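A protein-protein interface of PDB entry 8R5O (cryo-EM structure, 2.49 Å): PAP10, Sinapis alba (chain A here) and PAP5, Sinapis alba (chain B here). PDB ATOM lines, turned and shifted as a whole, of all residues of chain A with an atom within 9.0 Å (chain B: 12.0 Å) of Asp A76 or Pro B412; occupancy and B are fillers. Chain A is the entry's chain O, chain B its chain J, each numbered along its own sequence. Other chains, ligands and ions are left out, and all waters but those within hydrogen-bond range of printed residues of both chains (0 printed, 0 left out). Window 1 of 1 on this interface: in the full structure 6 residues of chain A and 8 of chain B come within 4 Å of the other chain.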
ATOM      1  N   VAL A  73      23.759 -29.401  21.488  1.00  0.00           N
ATOM      2  CA  VAL A  73      24.018 -28.181  20.732  1.00  0.00           C
ATOM      3  C   VAL A  73      23.086 -27.096  21.253  1.00  0.00           C
ATOM      4  O   VAL A  73      21.860 -27.231  21.167  1.00  0.00           O
ATOM      5  CB  VAL A  73      23.826 -28.389  19.222  1.00  0.00           C
ATOM      6  CG1 VAL A  73      24.109 -27.099  18.469  1.00  0.00           C
ATOM      7  CG2 VAL A  73      24.723 -29.511  18.721  1.00  0.00           C
ATOM      8  N   ARG A  74      23.668 -26.030  21.792  1.00  0.00           N
ATOM      9  CA  ARG A  74      22.881 -24.914  22.298  1.00  0.00           C
ATOM     10  C   ARG A  74      22.165 -24.206  21.154  1.00  0.00           C
ATOM     11  O   ARG A  74      22.727 -24.021  20.070  1.00  0.00           O
ATOM     12  CB  ARG A  74      23.787 -23.940  23.051  1.00  0.00           C
ATOM     13  CG  ARG A  74      23.092 -22.719  23.621  1.00  0.00           C
ATOM     14  CD  ARG A  74      22.044 -23.099  24.651  1.00  0.00           C
ATOM     15  NE  ARG A  74      21.625 -21.947  25.440  1.00  0.00           N
ATOM     16  CZ  ARG A  74      20.560 -21.922  26.228  1.00  0.00           C
ATOM     17  NH1 ARG A  74      19.760 -22.969  26.342  1.00  0.00           N
ATOM     18  NH2 ARG A  74      20.288 -20.818  26.917  1.00  0.00           N
ATOM     19  N   GLU A  75      20.916 -23.819  21.392  1.00  0.00           N
ATOM     20  CA  GLU A  75      20.153 -23.128  20.363  1.00  0.00           C
ATOM     21  C   GLU A  75      20.722 -21.733  20.124  1.00  0.00           C
ATOM     22  O   GLU A  75      21.288 -21.102  21.023  1.00  0.00           O
ATOM     23  CB  GLU A  75      18.674 -23.045  20.748  1.00  0.00           C
ATOM     24  CG  GLU A  75      18.307 -21.861  21.624  1.00  0.00           C
ATOM     25  CD  GLU A  75      18.814 -21.997  23.042  1.00  0.00           C
ATOM     26  OE1 GLU A  75      18.895 -23.138  23.539  1.00  0.00           O
ATOM     27  OE2 GLU A  75      19.131 -20.959  23.662  1.00  0.00           O
ATOM     28  N   ASP A  76      20.582 -21.259  18.886  1.00  0.00           N
ATOM     29  CA  ASP A  76      21.194 -20.003  18.474  1.00  0.00           C
ATOM     30  C   ASP A  76      20.356 -18.777  18.802  1.00  0.00           C
ATOM     31  O   ASP A  76      20.868 -17.658  18.699  1.00  0.00           O
ATOM     32  CB  ASP A  76      21.481 -20.033  16.970  1.00  0.00           C
ATOM     33  CG  ASP A  76      22.763 -20.769  16.636  1.00  0.00           C
ATOM     34  OD1 ASP A  76      23.787 -20.502  17.295  1.00  0.00           O
ATOM     35  OD2 ASP A  76      22.746 -21.612  15.714  1.00  0.00           O
ATOM     36  N   TYR A  77      19.094 -18.944  19.194  1.00  0.00           N
ATOM     37  CA  TYR A  77      18.202 -17.810  19.394  1.00  0.00           C
ATOM     38  C   TYR A  77      17.398 -17.994  20.669  1.00  0.00           C
ATOM     39  O   TYR A  77      16.803 -19.053  20.888  1.00  0.00           O
ATOM     40  CB  TYR A  77      17.271 -17.632  18.190  1.00  0.00           C
ATOM     41  CG  TYR A  77      18.020 -17.315  16.919  1.00  0.00           C
ATOM     42  CD1 TYR A  77      18.442 -16.022  16.646  1.00  0.00           C
ATOM     43  CD2 TYR A  77      18.322 -18.310  16.000  1.00  0.00           C
ATOM     44  CE1 TYR A  77      19.135 -15.726  15.492  1.00  0.00           C
ATOM     45  CE2 TYR A  77      19.013 -18.023  14.841  1.00  0.00           C
ATOM     46  CZ  TYR A  77      19.419 -16.729  14.593  1.00  0.00           C
ATOM     47  OH  TYR A  77      20.108 -16.436  13.441  1.00  0.00           O
ATOM     48  N   LEU A  78      17.373 -16.952  21.500  1.00  0.00           N
ATOM     49  CA  LEU A  78      16.712 -17.006  22.798  1.00  0.00           C
ATOM     50  C   LEU A  78      15.291 -16.458  22.773  1.00  0.00           C
ATOM     51  O   LEU A  78      14.451 -16.914  23.556  1.00  0.00           O
ATOM     52  CB  LEU A  78      17.531 -16.235  23.839  1.00  0.00           C
ATOM     53  CG  LEU A  78      18.649 -16.960  24.597  1.00  0.00           C
ATOM     54  CD1 LEU A  78      19.644 -17.614  23.654  1.00  0.00           C
ATOM     55  CD2 LEU A  78      19.361 -15.990  25.525  1.00  0.00           C
ATOM     56  N   VAL A  79      15.001 -15.496  21.904  1.00  0.00           N
ATOM     57  CA  VAL A  79      13.690 -14.853  21.886  1.00  0.00           C
ATOM     58  C   VAL A  79      12.695 -15.779  21.198  1.00  0.00           C
ATOM     59  O   VAL A  79      12.916 -16.213  20.062  1.00  0.00           O
ATOM     60  CB  VAL A  79      13.752 -13.488  21.188  1.00  0.00           C
ATOM     61  CG1 VAL A  79      12.370 -12.856  21.137  1.00  0.00           C
ATOM     62  CG2 VAL A  79      14.733 -12.573  21.901  1.00  0.00           C
ATOM     63  N   ALA A 115      16.098  -7.085  16.040  1.00  0.00           N
ATOM     64  CA  ALA A 115      16.207  -8.491  16.416  1.00  0.00           C
ATOM     65  C   ALA A 115      17.526  -8.777  17.121  1.00  0.00           C
ATOM     66  O   ALA A 115      17.571  -9.565  18.073  1.00  0.00           O
ATOM     67  CB  ALA A 115      16.055  -9.379  15.182  1.00  0.00           C
ATOM     68  N   GLU A 119      18.048 -10.045  21.217  1.00  0.00           N
ATOM     69  CA  GLU A 119      18.813 -11.240  21.559  1.00  0.00           C
ATOM     70  C   GLU A 119      19.884 -10.921  22.592  1.00  0.00           C
ATOM     71  O   GLU A 119      20.126 -11.708  23.513  1.00  0.00           O
ATOM     72  CB  GLU A 119      19.435 -11.851  20.304  1.00  0.00           C
ATOM     73  CG  GLU A 119      18.440 -12.534  19.378  1.00  0.00           C
ATOM     74  CD  GLU A 119      17.873 -13.817  19.962  1.00  0.00           C
ATOM     75  OE1 GLU A 119      18.488 -14.378  20.893  1.00  0.00           O
ATOM     76  OE2 GLU A 119      16.811 -14.267  19.486  1.00  0.00           O
ATOM     77  N   MET A 120      20.541  -9.766  22.453  1.00  0.00           N
ATOM     78  CA  MET A 120      21.501  -9.333  23.462  1.00  0.00           C
ATOM     79  C   MET A 120      20.810  -9.036  24.788  1.00  0.00           C
ATOM     80  O   MET A 120      21.343  -9.353  25.856  1.00  0.00           O
ATOM     81  CB  MET A 120      22.268  -8.107  22.963  1.00  0.00           C
ATOM     82  CG  MET A 120      23.164  -7.461  24.004  1.00  0.00           C
ATOM     83  SD  MET A 120      24.349  -8.610  24.732  1.00  0.00           S
ATOM     84  CE  MET A 120      25.260  -9.128  23.284  1.00  0.00           C
ATOM     85  N   VAL A 123      20.241 -12.208  26.653  1.00  0.00           N
ATOM     86  CA  VAL A 123      21.445 -12.725  27.297  1.00  0.00           C
ATOM     87  C   VAL A 123      21.700 -12.001  28.614  1.00  0.00           C
ATOM     88  O   VAL A 123      22.041 -12.627  29.623  1.00  0.00           O
ATOM     89  CB  VAL A 123      22.649 -12.620  26.346  1.00  0.00           C
ATOM     90  CG1 VAL A 123      23.926 -13.047  27.051  1.00  0.00           C
ATOM     91  CG2 VAL A 123      22.421 -13.463  25.104  1.00  0.00           C
ATOM     92  N   MET B 402      34.661  -7.517  14.990  1.00  0.00           N
ATOM     93  CA  MET B 402      33.663  -8.068  14.083  1.00  0.00           C
ATOM     94  C   MET B 402      32.612  -8.851  14.857  1.00  0.00           C
ATOM     95  O   MET B 402      32.940  -9.729  15.661  1.00  0.00           O
ATOM     96  CB  MET B 402      34.330  -8.964  13.042  1.00  0.00           C
ATOM     97  CG  MET B 402      35.354  -8.265  12.159  1.00  0.00           C
ATOM     98  SD  MET B 402      34.649  -7.011  11.069  1.00  0.00           S
ATOM     99  CE  MET B 402      34.976  -5.516  11.999  1.00  0.00           C
ATOM    100  N   ASP B 403      31.344  -8.528  14.613  1.00  0.00           N
ATOM    101  CA  ASP B 403      30.222  -9.227  15.227  1.00  0.00           C
ATOM    102  C   ASP B 403      29.817 -10.370  14.305  1.00  0.00           C
ATOM    103  O   ASP B 403      29.189 -10.147  13.265  1.00  0.00           O
ATOM    104  CB  ASP B 403      29.058  -8.269  15.473  1.00  0.00           C
ATOM    105  CG  ASP B 403      27.915  -8.915  16.237  1.00  0.00           C
ATOM    106  OD1 ASP B 403      28.054 -10.076  16.673  1.00  0.00           O
ATOM    107  OD2 ASP B 403      26.870  -8.255  16.404  1.00  0.00           O
ATOM    108  N   PHE B 404      30.171 -11.592  14.690  1.00  0.00           N
ATOM    109  CA  PHE B 404      29.938 -12.765  13.859  1.00  0.00           C
ATOM    110  C   PHE B 404      28.481 -13.206  13.839  1.00  0.00           C
ATOM    111  O   PHE B 404      28.158 -14.181  13.153  1.00  0.00           O
ATOM    112  CB  PHE B 404      30.831 -13.916  14.327  1.00  0.00           C
ATOM    113  CG  PHE B 404      32.296 -13.684  14.082  1.00  0.00           C
ATOM    114  CD1 PHE B 404      32.723 -13.001  12.957  1.00  0.00           C
ATOM    115  CD2 PHE B 404      33.243 -14.142  14.978  1.00  0.00           C
ATOM    116  CE1 PHE B 404      34.066 -12.784  12.727  1.00  0.00           C
ATOM    117  CE2 PHE B 404      34.591 -13.930  14.754  1.00  0.00           C
ATOM    118  CZ  PHE B 404      35.002 -13.250  13.626  1.00  0.00           C
ATOM    119  N   ARG B 405      27.598 -12.524  14.567  1.00  0.00           N
ATOM    120  CA  ARG B 405      26.165 -12.785  14.506  1.00  0.00           C
ATOM    121  C   ARG B 405      25.420 -11.719  13.710  1.00  0.00           C
ATOM    122  O   ARG B 405      24.202 -11.581  13.849  1.00  0.00           O
ATOM    123  CB  ARG B 405      25.583 -12.902  15.915  1.00  0.00           C
ATOM    124  CG  ARG B 405      26.148 -14.057  16.720  1.00  0.00           C
ATOM    125  CD  ARG B 405      25.936 -15.381  16.007  1.00  0.00           C
ATOM    126  NE  ARG B 405      24.536 -15.596  15.667  1.00  0.00           N
ATOM    127  CZ  ARG B 405      23.625 -16.082  16.499  1.00  0.00           C
ATOM    128  NH1 ARG B 405      23.934 -16.421  17.740  1.00  0.00           N
ATOM    129  NH2 ARG B 405      22.374 -16.230  16.077  1.00  0.00           N
ATOM    130  N   GLY B 406      26.131 -10.961  12.880  1.00  0.00           N
ATOM    131  CA  GLY B 406      25.518  -9.937  12.068  1.00  0.00           C
ATOM    132  C   GLY B 406      24.781 -10.514  10.881  1.00  0.00           C
ATOM    133  O   GLY B 406      24.878 -11.705  10.553  1.00  0.00           O
ATOM    134  N   PRO B 407      24.016  -9.651  10.208  1.00  0.00           N
ATOM    135  CA  PRO B 407      23.173 -10.123   9.096  1.00  0.00           C
ATOM    136  C   PRO B 407      23.950 -10.698   7.924  1.00  0.00           C
ATOM    137  O   PRO B 407      23.368 -11.442   7.127  1.00  0.00           O
ATOM    138  CB  PRO B 407      22.400  -8.862   8.684  1.00  0.00           C
ATOM    139  CG  PRO B 407      22.483  -7.952   9.863  1.00  0.00           C
ATOM    140  CD  PRO B 407      23.816  -8.221  10.483  1.00  0.00           C
ATOM    141  N   ASP B 408      25.235 -10.384   7.786  1.00  0.00           N
ATOM    142  CA  ASP B 408      26.030 -10.861   6.663  1.00  0.00           C
ATOM    143  C   ASP B 408      26.821 -12.123   6.986  1.00  0.00           C
ATOM    144  O   ASP B 408      27.689 -12.511   6.199  1.00  0.00           O
ATOM    145  CB  ASP B 408      26.980  -9.763   6.184  1.00  0.00           C
ATOM    146  CG  ASP B 408      26.247  -8.561   5.622  1.00  0.00           C
ATOM    147  OD1 ASP B 408      25.145  -8.741   5.063  1.00  0.00           O
ATOM    148  OD2 ASP B 408      26.773  -7.435   5.740  1.00  0.00           O
ATOM    149  N   PHE B 409      26.546 -12.768   8.114  1.00  0.00           N
ATOM    150  CA  PHE B 409      27.258 -13.968   8.524  1.00  0.00           C
ATOM    151  C   PHE B 409      26.322 -15.167   8.518  1.00  0.00           C
ATOM    152  O   PHE B 409      25.132 -15.042   8.822  1.00  0.00           O
ATOM    153  CB  PHE B 409      27.873 -13.800   9.915  1.00  0.00           C
ATOM    154  CG  PHE B 409      29.089 -12.927   9.935  1.00  0.00           C
ATOM    155  CD1 PHE B 409      30.328 -13.438   9.592  1.00  0.00           C
ATOM    156  CD2 PHE B 409      28.995 -11.594  10.296  1.00  0.00           C
ATOM    157  CE1 PHE B 409      31.450 -12.638   9.606  1.00  0.00           C
ATOM    158  CE2 PHE B 409      30.114 -10.789  10.311  1.00  0.00           C
ATOM    159  CZ  PHE B 409      31.343 -11.313   9.968  1.00  0.00           C
ATOM    160  N   HIS B 410      26.869 -16.325   8.165  1.00  0.00           N
ATOM    161  CA  HIS B 410      26.120 -17.567   8.228  1.00  0.00           C
ATOM    162  C   HIS B 410      25.885 -17.966   9.685  1.00  0.00           C
ATOM    163  O   HIS B 410      26.489 -17.424  10.614  1.00  0.00           O
ATOM    164  CB  HIS B 410      26.862 -18.675   7.482  1.00  0.00           C
ATOM    165  CG  HIS B 410      28.232 -18.951   8.018  1.00  0.00           C
ATOM    166  ND1 HIS B 410      28.450 -19.693   9.158  1.00  0.00           N
ATOM    167  CD2 HIS B 410      29.455 -18.575   7.575  1.00  0.00           C
ATOM    168  CE1 HIS B 410      29.748 -19.767   9.392  1.00  0.00           C
ATOM    169  NE2 HIS B 410      30.380 -19.099   8.445  1.00  0.00           N
ATOM    170  N   GLU B 411      24.992 -18.932   9.875  1.00  0.00           N
ATOM    171  CA  GLU B 411      24.687 -19.409  11.213  1.00  0.00           C
ATOM    172  C   GLU B 411      25.919 -20.070  11.833  1.00  0.00           C
ATOM    173  O   GLU B 411      26.753 -20.633  11.120  1.00  0.00           O
ATOM    174  CB  GLU B 411      23.523 -20.391  11.174  1.00  0.00           C
ATOM    175  CG  GLU B 411      22.229 -19.767  10.691  1.00  0.00           C
ATOM    176  CD  GLU B 411      21.798 -18.599  11.551  1.00  0.00           C
ATOM    177  OE1 GLU B 411      21.427 -18.825  12.721  1.00  0.00           O
ATOM    178  OE2 GLU B 411      21.845 -17.452  11.063  1.00  0.00           O
ATOM    179  N   PRO B 412      26.064 -19.994  13.157  1.00  0.00           N
ATOM    180  CA  PRO B 412      27.273 -20.523  13.799  1.00  0.00           C
ATOM    181  C   PRO B 412      27.481 -21.999  13.497  1.00  0.00           C
ATOM    182  O   PRO B 412      26.536 -22.791  13.484  1.00  0.00           O
ATOM    183  CB  PRO B 412      27.013 -20.286  15.291  1.00  0.00           C
ATOM    184  CG  PRO B 412      26.056 -19.146  15.323  1.00  0.00           C
ATOM    185  CD  PRO B 412      25.177 -19.320  14.120  1.00  0.00           C
ATOM    186  N   THR B 413      28.730 -22.360  13.253  1.00  0.00           N
ATOM    187  CA  THR B 413      29.065 -23.737  12.917  1.00  0.00           C
ATOM    188  C   THR B 413      29.025 -24.601  14.169  1.00  0.00           C
ATOM    189  O   THR B 413      29.750 -24.315  15.131  1.00  0.00           O
ATOM    190  CB  THR B 413      30.448 -23.805  12.272  1.00  0.00           C
ATOM    191  OG1 THR B 413      30.476 -22.970  11.108  1.00  0.00           O
ATOM    192  CG2 THR B 413      30.778 -25.233  11.870  1.00  0.00           C
ATOM    193  N   PRO B 414      28.206 -25.647  14.211  1.00  0.00           N
ATOM    194  CA  PRO B 414      28.190 -26.519  15.387  1.00  0.00           C
ATOM    195  C   PRO B 414      29.433 -27.389  15.454  1.00  0.00           C
ATOM    196  O   PRO B 414      30.066 -27.693  14.440  1.00  0.00           O
ATOM    197  CB  PRO B 414      26.931 -27.367  15.180  1.00  0.00           C
ATOM    198  CG  PRO B 414      26.780 -27.427  13.696  1.00  0.00           C
ATOM    199  CD  PRO B 414      27.250 -26.089  13.180  1.00  0.00           C
ATOM    200  N   ASN B 415      29.788 -27.784  16.675  1.00  0.00           N
ATOM    201  CA  ASN B 415      30.838 -28.778  16.850  1.00  0.00           C
ATOM    202  C   ASN B 415      30.401 -30.092  16.221  1.00  0.00           C
ATOM    203  O   ASN B 415      29.269 -30.540  16.421  1.00  0.00           O
ATOM    204  CB  ASN B 415      31.150 -28.970  18.334  1.00  0.00           C
ATOM    205  CG  ASN B 415      32.215 -30.022  18.572  1.00  0.00           C
ATOM    206  OD1 ASN B 415      31.920 -31.136  19.002  1.00  0.00           O
ATOM    207  ND2 ASN B 415      33.463 -29.674  18.284  1.00  0.00           N
ATOM    208  N   MET B 416      31.299 -30.704  15.446  1.00  0.00           N
ATOM    209  CA  MET B 416      30.916 -31.872  14.660  1.00  0.00           C
ATOM    210  C   MET B 416      30.470 -33.024  15.549  1.00  0.00           C
ATOM    211  O   MET B 416      29.468 -33.687  15.261  1.00  0.00           O
ATOM    212  CB  MET B 416      32.070 -32.309  13.761  1.00  0.00           C
ATOM    213  CG  MET B 416      31.797 -33.605  13.016  1.00  0.00           C
ATOM    214  SD  MET B 416      30.345 -33.517  11.951  1.00  0.00           S
ATOM    215  CE  MET B 416      31.056 -32.826  10.462  1.00  0.00           C
ATOM    216  N   LEU B 417      31.200 -33.276  16.637  1.00  0.00           N
ATOM    217  CA  LEU B 417      30.824 -34.355  17.545  1.00  0.00           C
ATOM    218  C   LEU B 417      29.480 -34.074  18.201  1.00  0.00           C
ATOM    219  O   LEU B 417      28.605 -34.946  18.250  1.00  0.00           O
ATOM    220  CB  LEU B 417      31.912 -34.555  18.600  1.00  0.00           C
ATOM    221  CG  LEU B 417      31.706 -35.747  19.535  1.00  0.00           C
ATOM    222  CD1 LEU B 417      31.714 -37.045  18.747  1.00  0.00           C
ATOM    223  CD2 LEU B 417      32.761 -35.770  20.630  1.00  0.00           C
ATOM    224  N   SER B 418      29.290 -32.851  18.704  1.00  0.00           N
ATOM    225  CA  SER B 418      28.016 -32.497  19.321  1.00  0.00           C
ATOM    226  C   SER B 418      26.879 -32.517  18.310  1.00  0.00           C
ATOM    227  O   SER B 418      25.731 -32.797  18.671  1.00  0.00           O
ATOM    228  CB  SER B 418      28.112 -31.124  19.984  1.00  0.00           C
ATOM    229  OG  SER B 418      29.035 -31.142  21.059  1.00  0.00           O
ATOM    230  N   TYR B 419      27.175 -32.222  17.044  1.00  0.00           N
ATOM    231  CA  TYR B 419      26.143 -32.275  16.015  1.00  0.00           C
ATOM    232  C   TYR B 419      25.737 -33.712  15.716  1.00  0.00           C
ATOM    233  O   TYR B 419      24.547 -34.003  15.540  1.00  0.00           O
ATOM    234  CB  TYR B 419      26.636 -31.576  14.749  1.00  0.00           C
ATOM    235  CG  TYR B 419      25.570 -31.375  13.699  1.00  0.00           C
ATOM    236  CD1 TYR B 419      24.612 -30.383  13.837  1.00  0.00           C
ATOM    237  CD2 TYR B 419      25.529 -32.171  12.564  1.00  0.00           C
ATOM    238  CE1 TYR B 419      23.639 -30.194  12.879  1.00  0.00           C
ATOM    239  CE2 TYR B 419      24.559 -31.988  11.601  1.00  0.00           C
ATOM    240  CZ  TYR B 419      23.616 -30.997  11.764  1.00  0.00           C
ATOM    241  OH  TYR B 419      22.646 -30.808  10.808  1.00  0.00           O
ATOM    242  N   GLU B 422      23.726 -34.914  18.662  1.00  0.00           N
ATOM    243  CA  GLU B 422      22.408 -34.286  18.664  1.00  0.00           C
ATOM    244  C   GLU B 422      21.452 -35.001  17.718  1.00  0.00           C
ATOM    245  O   GLU B 422      20.278 -35.203  18.047  1.00  0.00           O
ATOM    246  CB  GLU B 422      22.530 -32.808  18.286  1.00  0.00           C
ATOM    247  CG  GLU B 422      21.221 -32.039  18.339  1.00  0.00           C
ATOM    248  CD  GLU B 422      20.865 -31.587  19.740  1.00  0.00           C
ATOM    249  OE1 GLU B 422      21.789 -31.413  20.562  1.00  0.00           O
ATOM    250  OE2 GLU B 422      19.663 -31.404  20.021  1.00  0.00           O
ATOM    251  N   ASN B 423      21.934 -35.395  16.543  1.00  0.00           N
ATOM    252  CA  ASN B 423      21.116 -36.079  15.552  1.00  0.00           C
ATOM    253  C   ASN B 423      21.077 -37.590  15.760  1.00  0.00           C
ATOM    254  O   ASN B 423      20.592 -38.309  14.881  1.00  0.00           O
ATOM    255  CB  ASN B 423      21.615 -35.756  14.142  1.00  0.00           C
ATOM    256  CG  ASN B 423      21.258 -34.348  13.709  1.00  0.00           C
ATOM    257  OD1 ASN B 423      20.251 -34.132  13.036  1.00  0.00           O
ATOM    258  ND2 ASN B 423      22.080 -33.381  14.099  1.00  0.00           N
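Of the 11 printed residues of chain A, 3 touch a printed residue of chain B. Hydrophobic or aromatic side chains of chain A that line the printed part of chain B: Val A73 and Tyr A77. Hydrophobic or aromatic side chains of chain B within 4 Å of the printed part of chain A: Pro B412. Among the printed residues, 6 pairs touch across the chains. Among the printed residues, no Asp or Glu carboxylate lies within 4 Å of a Lys or Arg side-chain nitrogen of the other chain.
Asp A76 touches just these residues of chain B: Arg B405 (3.3 Å) and Pro B412 (3.3 Å). Pro B412 touches just one residue of chain A: Asp A76 (3.3 Å). Tyr A77 touches just these residues of chain B: Arg B405 and Glu B411. No residue of chain B comes within 4 Å of Leu A78. Glu B411 touches just one residue of chain A: Tyr A77 (2.8 Å). No residue of chain A comes within 4 Å of Thr B413. Of the printed residues of chain A, Arg B405 touches Asp A76 and Tyr A77. Of the printed residues of chain A, Ser B418 touches Val A73. Of the printed residues of chain A, Glu B422 touches Val A73. Printed residues of chain B within 4 Å of Val A73: Ser B418 (3.4 Å) and Glu B422 (3.0 Å). Tyr B419 touches none of the printed residues of chain A. The nearest residue of chain A that does not touch Pro B412 is Tyr A77 (5.9 Å).
N of Val A73 sits at hydrogen-bond distance from OE1 of Glu B422 (3.0 Å). The guanidinium group (NH2) of Arg B405 is in hydrogen-bond range of the backbone carbonyl oxygen (O) of Asp A76, at 3.3 Å. OH of Tyr A77 lies close to NH2 of Arg B405 (3.5 Å). The side-chain carboxylate (OE1) of Glu B411 lies within hydrogen-bond range of the side-chain hydroxyl (OH) of Tyr A77 (2.8 Å).
Among the printed residues, pairs that only touch across the chains: Asp A76 with Pro B412 and Val A73 with Ser B418.
The side-chain carboxylate of Asp B403 sits close to the backbone NH of Arg B405. The side-chain amide oxygen (OD1) of Asn B415 sits at hydrogen-bond distance from the backbone NH (N) of Ser B418.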
